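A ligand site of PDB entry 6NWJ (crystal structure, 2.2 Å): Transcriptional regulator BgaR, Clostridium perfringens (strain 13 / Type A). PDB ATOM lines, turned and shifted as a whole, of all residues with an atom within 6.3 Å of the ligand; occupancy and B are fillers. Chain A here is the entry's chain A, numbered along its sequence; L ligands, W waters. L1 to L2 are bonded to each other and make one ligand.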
ATOM      1  N   GLN A   2       0.764  -4.263   2.677  1.00  0.00           N
ATOM      2  CA  GLN A   2       1.564  -3.950   3.874  1.00  0.00           C
ATOM      3  C   GLN A   2       2.932  -4.607   3.698  1.00  0.00           C
ATOM      4  O   GLN A   2       2.969  -5.759   3.285  1.00  0.00           O
ATOM      5  CB  GLN A   2       0.847  -4.454   5.129  1.00  0.00           C
ATOM      6  CG  GLN A   2      -0.447  -3.696   5.430  1.00  0.00           C
ATOM      7  CD  GLN A   2      -1.620  -4.170   4.611  1.00  0.00           C
ATOM      8  OE1 GLN A   2      -1.544  -5.196   3.939  1.00  0.00           O
ATOM      9  NE2 GLN A   2      -2.711  -3.434   4.664  1.00  0.00           N
ATOM     10  N   TRP A   5       2.282  -7.272   8.347  1.00  0.00           N
ATOM     11  CA  TRP A   5       1.011  -7.299   9.109  1.00  0.00           C
ATOM     12  C   TRP A   5       0.942  -8.636   9.834  1.00  0.00           C
ATOM     13  O   TRP A   5       0.278  -9.533   9.338  1.00  0.00           O
ATOM     14  CB  TRP A   5      -0.222  -7.024   8.230  1.00  0.00           C
ATOM     15  CG  TRP A   5      -1.432  -6.635   9.015  1.00  0.00           C
ATOM     16  CD1 TRP A   5      -1.568  -6.674  10.375  1.00  0.00           C
ATOM     17  CD2 TRP A   5      -2.688  -6.130   8.508  1.00  0.00           C
ATOM     18  NE1 TRP A   5      -2.805  -6.217  10.750  1.00  0.00           N
ATOM     19  CE2 TRP A   5      -3.517  -5.872   9.630  1.00  0.00           C
ATOM     20  CE3 TRP A   5      -3.184  -5.847   7.228  1.00  0.00           C
ATOM     21  CZ2 TRP A   5      -4.820  -5.384   9.518  1.00  0.00           C
ATOM     22  CZ3 TRP A   5      -4.467  -5.357   7.105  1.00  0.00           C
ATOM     23  CH2 TRP A   5      -5.270  -5.127   8.234  1.00  0.00           C
ATOM     24  N   LYS A   7      -0.479 -10.808  12.601  1.00  0.00           N
ATOM     25  CA  LYS A   7      -1.636 -10.965  13.529  1.00  0.00           C
ATOM     26  C   LYS A   7      -1.307 -12.105  14.500  1.00  0.00           C
ATOM     27  O   LYS A   7      -0.877 -13.145  14.010  1.00  0.00           O
ATOM     28  CB  LYS A   7      -2.927 -11.181  12.749  1.00  0.00           C
ATOM     29  CG  LYS A   7      -3.288 -10.025  11.838  1.00  0.00           C
ATOM     30  CD  LYS A   7      -4.670 -10.125  11.247  1.00  0.00           C
ATOM     31  CE  LYS A   7      -5.052  -8.923  10.400  1.00  0.00           C
ATOM     32  NZ  LYS A   7      -4.419  -8.972   9.065  1.00  0.00           N
ATOM     33  N   GLU A  19      -1.328  -7.512  17.268  1.00  0.00           N
ATOM     34  CA  GLU A  19      -0.738  -7.409  15.913  1.00  0.00           C
ATOM     35  C   GLU A  19       0.332  -6.329  15.888  1.00  0.00           C
ATOM     36  O   GLU A  19       0.295  -5.430  16.758  1.00  0.00           O
ATOM     37  CB  GLU A  19      -1.817  -7.093  14.867  1.00  0.00           C
ATOM     38  CG  GLU A  19      -2.545  -5.769  15.081  1.00  0.00           C
ATOM     39  CD  GLU A  19      -3.672  -5.451  14.092  1.00  0.00           C
ATOM     40  OE1 GLU A  19      -4.442  -6.359  13.733  1.00  0.00           O
ATOM     41  OE2 GLU A  19      -3.785  -4.277  13.676  1.00  0.00           O
ATOM     42  N   GLU A  23       3.153  -0.061   7.082  1.00  0.00           N
ATOM     43  CA  GLU A  23       2.455   0.249   5.813  1.00  0.00           C
ATOM     44  C   GLU A  23       2.967   1.561   5.237  1.00  0.00           C
ATOM     45  O   GLU A  23       2.932   2.600   5.924  1.00  0.00           O
ATOM     46  CB  GLU A  23       0.939   0.340   6.019  1.00  0.00           C
ATOM     47  CG  GLU A  23       0.216   0.598   4.722  1.00  0.00           C
ATOM     48  CD  GLU A  23      -1.267   0.332   4.773  1.00  0.00           C
ATOM     49  OE1 GLU A  23      -1.691  -0.516   5.593  1.00  0.00           O
ATOM     50  OE2 GLU A  23      -2.002   0.985   3.990  1.00  0.00           O
ATOM     51  N   TYR A  31      -8.133   4.918   4.993  1.00  0.00           N
ATOM     52  CA  TYR A  31      -9.145   4.016   5.582  1.00  0.00           C
ATOM     53  C   TYR A  31     -10.120   4.904   6.330  1.00  0.00           C
ATOM     54  O   TYR A  31      -9.727   5.969   6.836  1.00  0.00           O
ATOM     55  CB  TYR A  31      -8.458   2.963   6.462  1.00  0.00           C
ATOM     56  CG  TYR A  31      -7.354   2.256   5.731  1.00  0.00           C
ATOM     57  CD1 TYR A  31      -7.626   1.221   4.842  1.00  0.00           C
ATOM     58  CD2 TYR A  31      -6.045   2.683   5.841  1.00  0.00           C
ATOM     59  CE1 TYR A  31      -6.614   0.595   4.132  1.00  0.00           C
ATOM     60  CE2 TYR A  31      -5.017   2.088   5.119  1.00  0.00           C
ATOM     61  CZ  TYR A  31      -5.312   1.043   4.263  1.00  0.00           C
ATOM     62  OH  TYR A  31      -4.284   0.464   3.583  1.00  0.00           O
ATOM     63  N   ASN A  32     -11.361   4.441   6.379  1.00  0.00           N
ATOM     64  CA  ASN A  32     -12.514   5.170   6.956  1.00  0.00           C
ATOM     65  C   ASN A  32     -13.421   4.091   7.525  1.00  0.00           C
ATOM     66  O   ASN A  32     -13.997   3.334   6.698  1.00  0.00           O
ATOM     67  CB  ASN A  32     -13.211   6.019   5.902  1.00  0.00           C
ATOM     68  CG  ASN A  32     -14.337   6.855   6.481  1.00  0.00           C
ATOM     69  OD1 ASN A  32     -14.887   6.507   7.515  1.00  0.00           O
ATOM     70  ND2 ASN A  32     -14.641   7.972   5.846  1.00  0.00           N
ATOM     71  N   TYR A  33     -13.475   3.934   8.840  1.00  0.00           N
ATOM     72  CA  TYR A  33     -14.199   2.803   9.474  1.00  0.00           C
ATOM     73  C   TYR A  33     -14.373   3.094  10.956  1.00  0.00           C
ATOM     74  O   TYR A  33     -13.689   4.002  11.534  1.00  0.00           O
ATOM     75  CB  TYR A  33     -13.454   1.487   9.185  1.00  0.00           C
ATOM     76  CG  TYR A  33     -12.096   1.355   9.827  1.00  0.00           C
ATOM     77  CD1 TYR A  33     -10.948   1.875   9.214  1.00  0.00           C
ATOM     78  CD2 TYR A  33     -11.941   0.709  11.047  1.00  0.00           C
ATOM     79  CE1 TYR A  33      -9.693   1.747   9.791  1.00  0.00           C
ATOM     80  CE2 TYR A  33     -10.700   0.567  11.634  1.00  0.00           C
ATOM     81  CZ  TYR A  33      -9.562   1.081  11.008  1.00  0.00           C
ATOM     82  OH  TYR A  33      -8.351   0.933  11.607  1.00  0.00           O
ATOM     83  N   GLU A  34     -15.309   2.363  11.557  1.00  0.00           N
ATOM     84  CA  GLU A  34     -15.445   2.270  13.029  1.00  0.00           C
ATOM     85  C   GLU A  34     -14.452   1.219  13.537  1.00  0.00           C
ATOM     86  O   GLU A  34     -14.520   0.063  13.096  1.00  0.00           O
ATOM     87  CB  GLU A  34     -16.882   1.937  13.409  1.00  0.00           C
ATOM     88  CG  GLU A  34     -17.100   1.978  14.910  1.00  0.00           C
ATOM     89  CD  GLU A  34     -18.527   1.626  15.297  1.00  0.00           C
ATOM     90  OE1 GLU A  34     -19.402   2.488  15.131  1.00  0.00           O
ATOM     91  OE2 GLU A  34     -18.743   0.497  15.754  1.00  0.00           O
ATOM     92  N   VAL A  35     -13.558   1.605  14.444  1.00  0.00           N
ATOM     93  CA  VAL A  35     -12.499   0.714  15.002  1.00  0.00           C
ATOM     94  C   VAL A  35     -13.165  -0.441  15.780  1.00  0.00           C
ATOM     95  O   VAL A  35     -14.068  -0.170  16.575  1.00  0.00           O
ATOM     96  CB  VAL A  35     -11.526   1.508  15.887  1.00  0.00           C
ATOM     97  CG1 VAL A  35     -10.458   0.590  16.489  1.00  0.00           C
ATOM     98  CG2 VAL A  35     -10.896   2.669  15.121  1.00  0.00           C
ATOM     99  N   LEU A  36     -12.762  -1.681  15.481  1.00  0.00           N
ATOM    100  CA  LEU A  36     -13.273  -2.928  16.110  1.00  0.00           C
ATOM    101  C   LEU A  36     -12.256  -3.448  17.137  1.00  0.00           C
ATOM    102  O   LEU A  36     -12.683  -3.988  18.155  1.00  0.00           O
ATOM    103  CB  LEU A  36     -13.505  -3.993  15.046  1.00  0.00           C
ATOM    104  CG  LEU A  36     -14.464  -3.627  13.929  1.00  0.00           C
ATOM    105  CD1 LEU A  36     -14.542  -4.773  12.937  1.00  0.00           C
ATOM    106  CD2 LEU A  36     -15.841  -3.260  14.467  1.00  0.00           C
ATOM    107  N   LYS A  37     -10.965  -3.296  16.835  1.00  0.00           N
ATOM    108  CA  LYS A  37      -9.869  -3.755  17.711  1.00  0.00           C
ATOM    109  C   LYS A  37      -9.834  -2.925  18.992  1.00  0.00           C
ATOM    110  O   LYS A  37     -10.405  -1.826  19.031  1.00  0.00           O
ATOM    111  CB  LYS A  37      -8.562  -3.720  16.922  1.00  0.00           C
ATOM    112  CG  LYS A  37      -8.553  -4.816  15.864  1.00  0.00           C
ATOM    113  CD  LYS A  37      -7.620  -4.621  14.726  1.00  0.00           C
ATOM    114  CE  LYS A  37      -7.793  -5.719  13.714  1.00  0.00           C
ATOM    115  NZ  LYS A  37      -6.893  -5.533  12.560  1.00  0.00           N
ATOM    116  N   VAL A  40      -4.892   0.414  19.068  1.00  0.00           N
ATOM    117  CA  VAL A  40      -3.851   0.308  18.033  1.00  0.00           C
ATOM    118  C   VAL A  40      -3.101   1.632  17.953  1.00  0.00           C
ATOM    119  O   VAL A  40      -3.654   2.622  17.412  1.00  0.00           O
ATOM    120  CB  VAL A  40      -4.415  -0.112  16.669  1.00  0.00           C
ATOM    121  CG1 VAL A  40      -3.292  -0.514  15.740  1.00  0.00           C
ATOM    122  CG2 VAL A  40      -5.449  -1.236  16.778  1.00  0.00           C
ATOM    123  N   HIS A  42      -0.284   3.919  16.348  1.00  0.00           N
ATOM    124  CA  HIS A  42       0.461   4.154  15.083  1.00  0.00           C
ATOM    125  C   HIS A  42       1.537   5.202  15.325  1.00  0.00           C
ATOM    126  O   HIS A  42       1.230   6.195  16.002  1.00  0.00           O
ATOM    127  CB  HIS A  42      -0.495   4.617  13.987  1.00  0.00           C
ATOM    128  CG  HIS A  42      -1.512   3.604  13.598  1.00  0.00           C
ATOM    129  ND1 HIS A  42      -2.516   3.197  14.448  1.00  0.00           N
ATOM    130  CD2 HIS A  42      -1.728   2.954  12.427  1.00  0.00           C
ATOM    131  CE1 HIS A  42      -3.284   2.326  13.820  1.00  0.00           C
ATOM    132  NE2 HIS A  42      -2.828   2.153  12.598  1.00  0.00           N
ATOM    133  N   PHE A  66      -0.864   8.455  16.606  1.00  0.00           N
ATOM    134  CA  PHE A  66      -2.334   8.472  16.740  1.00  0.00           C
ATOM    135  C   PHE A  66      -2.737   7.095  17.242  1.00  0.00           C
ATOM    136  O   PHE A  66      -2.055   6.109  16.921  1.00  0.00           O
ATOM    137  CB  PHE A  66      -2.979   8.909  15.418  1.00  0.00           C
ATOM    138  CG  PHE A  66      -2.820   8.010  14.223  1.00  0.00           C
ATOM    139  CD1 PHE A  66      -1.777   8.183  13.330  1.00  0.00           C
ATOM    140  CD2 PHE A  66      -3.779   7.035  13.945  1.00  0.00           C
ATOM    141  CE1 PHE A  66      -1.667   7.387  12.205  1.00  0.00           C
ATOM    142  CE2 PHE A  66      -3.682   6.240  12.814  1.00  0.00           C
ATOM    143  CZ  PHE A  66      -2.626   6.420  11.948  1.00  0.00           C
ATOM    144  N   LEU A  68      -5.952   4.301  17.868  1.00  0.00           N
ATOM    145  CA  LEU A  68      -7.318   3.843  17.539  1.00  0.00           C
ATOM    146  C   LEU A  68      -7.812   3.045  18.738  1.00  0.00           C
ATOM    147  O   LEU A  68      -7.061   2.175  19.207  1.00  0.00           O
ATOM    148  CB  LEU A  68      -7.257   2.966  16.292  1.00  0.00           C
ATOM    149  CG  LEU A  68      -6.529   3.586  15.098  1.00  0.00           C
ATOM    150  CD1 LEU A  68      -6.651   2.684  13.891  1.00  0.00           C
ATOM    151  CD2 LEU A  68      -7.038   4.994  14.803  1.00  0.00           C
ATOM    152  N   TYR A  76      -8.084   7.985   8.182  1.00  0.00           N
ATOM    153  CA  TYR A  76      -6.657   8.349   8.088  1.00  0.00           C
ATOM    154  C   TYR A  76      -6.185   8.047   6.666  1.00  0.00           C
ATOM    155  O   TYR A  76      -6.456   6.916   6.164  1.00  0.00           O
ATOM    156  CB  TYR A  76      -5.826   7.716   9.214  1.00  0.00           C
ATOM    157  CG  TYR A  76      -5.971   6.233   9.482  1.00  0.00           C
ATOM    158  CD1 TYR A  76      -7.077   5.719  10.161  1.00  0.00           C
ATOM    159  CD2 TYR A  76      -4.969   5.348   9.160  1.00  0.00           C
ATOM    160  CE1 TYR A  76      -7.206   4.370  10.445  1.00  0.00           C
ATOM    161  CE2 TYR A  76      -5.075   3.994   9.427  1.00  0.00           C
ATOM    162  CZ  TYR A  76      -6.204   3.492  10.071  1.00  0.00           C
ATOM    163  OH  TYR A  76      -6.287   2.150  10.377  1.00  0.00           O
ATOM    164  N   TYR A  86       3.696   4.312   8.288  1.00  0.00           N
ATOM    165  CA  TYR A  86       3.497   4.158   9.745  1.00  0.00           C
ATOM    166  C   TYR A  86       3.718   2.698  10.176  1.00  0.00           C
ATOM    167  O   TYR A  86       3.595   1.753   9.360  1.00  0.00           O
ATOM    168  CB  TYR A  86       2.159   4.746  10.158  1.00  0.00           C
ATOM    169  CG  TYR A  86       0.935   4.265   9.418  1.00  0.00           C
ATOM    170  CD1 TYR A  86       0.538   2.939   9.450  1.00  0.00           C
ATOM    171  CD2 TYR A  86       0.114   5.169   8.777  1.00  0.00           C
ATOM    172  CE1 TYR A  86      -0.622   2.506   8.827  1.00  0.00           C
ATOM    173  CE2 TYR A  86      -1.047   4.760   8.144  1.00  0.00           C
ATOM    174  CZ  TYR A  86      -1.418   3.422   8.167  1.00  0.00           C
ATOM    175  OH  TYR A  86      -2.553   3.048   7.521  1.00  0.00           O
ATOM    176  N   TRP A  88       2.605   0.110  13.485  1.00  0.00           N
ATOM    177  CA  TRP A  88       1.542   0.031  14.524  1.00  0.00           C
ATOM    178  C   TRP A  88       1.678  -1.220  15.372  1.00  0.00           C
ATOM    179  O   TRP A  88       2.218  -2.230  14.886  1.00  0.00           O
ATOM    180  CB  TRP A  88       0.146   0.137  13.910  1.00  0.00           C
ATOM    181  CG  TRP A  88      -0.352  -1.068  13.194  1.00  0.00           C
ATOM    182  CD1 TRP A  88      -1.058  -2.113  13.718  1.00  0.00           C
ATOM    183  CD2 TRP A  88      -0.269  -1.308  11.778  1.00  0.00           C
ATOM    184  NE1 TRP A  88      -1.385  -3.003  12.725  1.00  0.00           N
ATOM    185  CE2 TRP A  88      -0.922  -2.534  11.529  1.00  0.00           C
ATOM    186  CE3 TRP A  88       0.270  -0.604  10.703  1.00  0.00           C
ATOM    187  CZ2 TRP A  88      -1.023  -3.066  10.247  1.00  0.00           C
ATOM    188  CZ3 TRP A  88       0.180  -1.131   9.433  1.00  0.00           C
ATOM    189  CH2 TRP A  88      -0.469  -2.355   9.212  1.00  0.00           C
HETATM  190  C1  LIG L   1      -9.772  -3.653  10.574  1.00  0.00           C
HETATM  191  C2  LIG L   1      -8.614  -2.641  10.485  1.00  0.00           C
HETATM  192  C3  LIG L   1      -8.382  -2.226   9.038  1.00  0.00           C
HETATM  193  C4  LIG L   1      -9.688  -1.802   8.409  1.00  0.00           C
HETATM  194  C5  LIG L   1      -9.504  -1.584   6.913  1.00  0.00           C
HETATM  195  C6  LIG L   1     -11.023  -3.109   9.884  1.00  0.00           C
HETATM  196  O1  LIG L   1     -12.139  -4.022   9.916  1.00  0.00           O
HETATM  197  O2  LIG L   1     -10.139  -3.891  11.931  1.00  0.00           O
HETATM  198  O3  LIG L   1      -7.406  -3.178  11.009  1.00  0.00           O
HETATM  199  O4  LIG L   1      -7.568  -1.068   8.928  1.00  0.00           O
HETATM  200  O5  LIG L   1     -10.681  -2.796   8.531  1.00  0.00           O
HETATM  201  O6  LIG L   1     -10.596  -0.770   6.466  1.00  0.00           O
HETATM  202  C1  LG2 L   2      -6.187  -1.289   9.130  1.00  0.00           C
HETATM  203  C2  LG2 L   2      -5.350  -0.398   8.221  1.00  0.00           C
HETATM  204  C3  LG2 L   2      -3.876  -0.548   8.513  1.00  0.00           C
HETATM  205  C4  LG2 L   2      -3.618  -0.362   9.988  1.00  0.00           C
HETATM  206  C5  LG2 L   2      -4.533  -1.300  10.775  1.00  0.00           C
HETATM  207  C6  LG2 L   2      -4.395  -1.227  12.282  1.00  0.00           C
HETATM  208  O1  LG2 L   2      -5.551  -0.877   6.899  1.00  0.00           O
HETATM  209  O2  LG2 L   2      -3.142   0.388   7.715  1.00  0.00           O
HETATM  210  O3  LG2 L   2      -3.888   0.997  10.280  1.00  0.00           O
HETATM  211  O4  LG2 L   2      -5.894  -1.008  10.492  1.00  0.00           O
HETATM  212  O5  LG2 L   2      -5.328  -2.154  12.863  1.00  0.00           O
HETATM  213  O   HOH W   1      -7.138  -2.989   5.738  1.00  0.00           O
HETATM  214  O   HOH W   2     -11.393   1.782   5.252  1.00  0.00           O
HETATM  215  O   HOH W   3      -7.778  -0.899  13.596  1.00  0.00           O
HETATM  216  O   HOH W   4     -11.016  -6.306  12.123  1.00  0.00           O
HETATM  217  O   HOH W   5     -10.326  -2.113  13.932  1.00  0.00           O
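Water W5 lies within hydrogen-bond range of O2 of LIG L1, N of Leu 36 and N of Lys 37. Water W3 lies within hydrogen-bond range of OH of Tyr 33 (2.8 Å) and O5 of LG2 L2 (2.8 Å). Water W2 lies within hydrogen-bond range of the backbone NH (N) of Asn 32 (2.9 Å) and an oxygen (O6) of LIG L1 (2.9 Å).
OH of Tyr 76 sits at hydrogen-bond distance from O3 of LG2 L2 (2.7 Å). The side-chain carboxylate (OE1) of Glu 23 is in hydrogen-bond range of an oxygen (O2) of LG2 L2. An oxygen (O2) of LG2 L2 sits at hydrogen-bond distance from the side-chain hydroxyl of Tyr 86 (2.7 Å). The side-chain carboxylate (OE2) of Glu 19 sits at hydrogen-bond distance from an oxygen (O5) of LG2 L2, 2.7 Å away. An oxygen (O3) of LG2 L2 lies within hydrogen-bond range of a ring nitrogen (NE2) of His 42 (2.8 Å). The side-chain amino group (NZ) of Lys 37 lies within hydrogen-bond range of an oxygen (O3) of LIG L1. O4 of LG2 L2 is in hydrogen-bond range of OH of Tyr 33.
The side-chain hydroxyl (OH) of Tyr 76 lies within hydrogen-bond range of the side-chain hydroxyl (OH) of Tyr 33, 2.7 Å away. The backbone carbonyl oxygen (O) of Tyr 86 sits at hydrogen-bond distance from the backbone NH (N) of Glu 23, 2.9 Å away. The side-chain carboxylate (OE1) of Glu 23 sits close to the side-chain hydroxyl (OH) of Tyr 31 (3.4 Å). The side-chain amide nitrogen (NE2) of Gln 2 is in hydrogen-bond range of the side-chain carboxylate (OE1) of Glu 23. The indole nitrogen (NE1) of Trp 88 is in hydrogen-bond range of the side-chain carboxylate (OE2) of Glu 19 (2.9 Å). ND1 of His 42 lies within hydrogen-bond range of O of Val 40, at 3.2 Å. N of His 42 lies within hydrogen-bond range of O of Phe 66. N of Val 40 sits at hydrogen-bond distance from O of Leu 68 (2.8 Å).
Residues that only touch the ligand: Trp 5, Tyr 31, Leu 36, Val 40 and Trp 88. Hydrophobic or aromatic side chains that line the ligand: Trp 5, Tyr 31, Tyr 33, Leu 36, Val 40, His 42, Tyr 76, Tyr 86 and Trp 88. Within 4 Å of the ligand: Trp 5, Glu 19, Glu 23, Tyr 31, Tyr 33, Leu 36, Lys 37, Val 40, His 42, Tyr 76, Tyr 86 and Trp 88. The nearest printed residue that does not touch the ligand is Gln 2 (4.4 Å).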
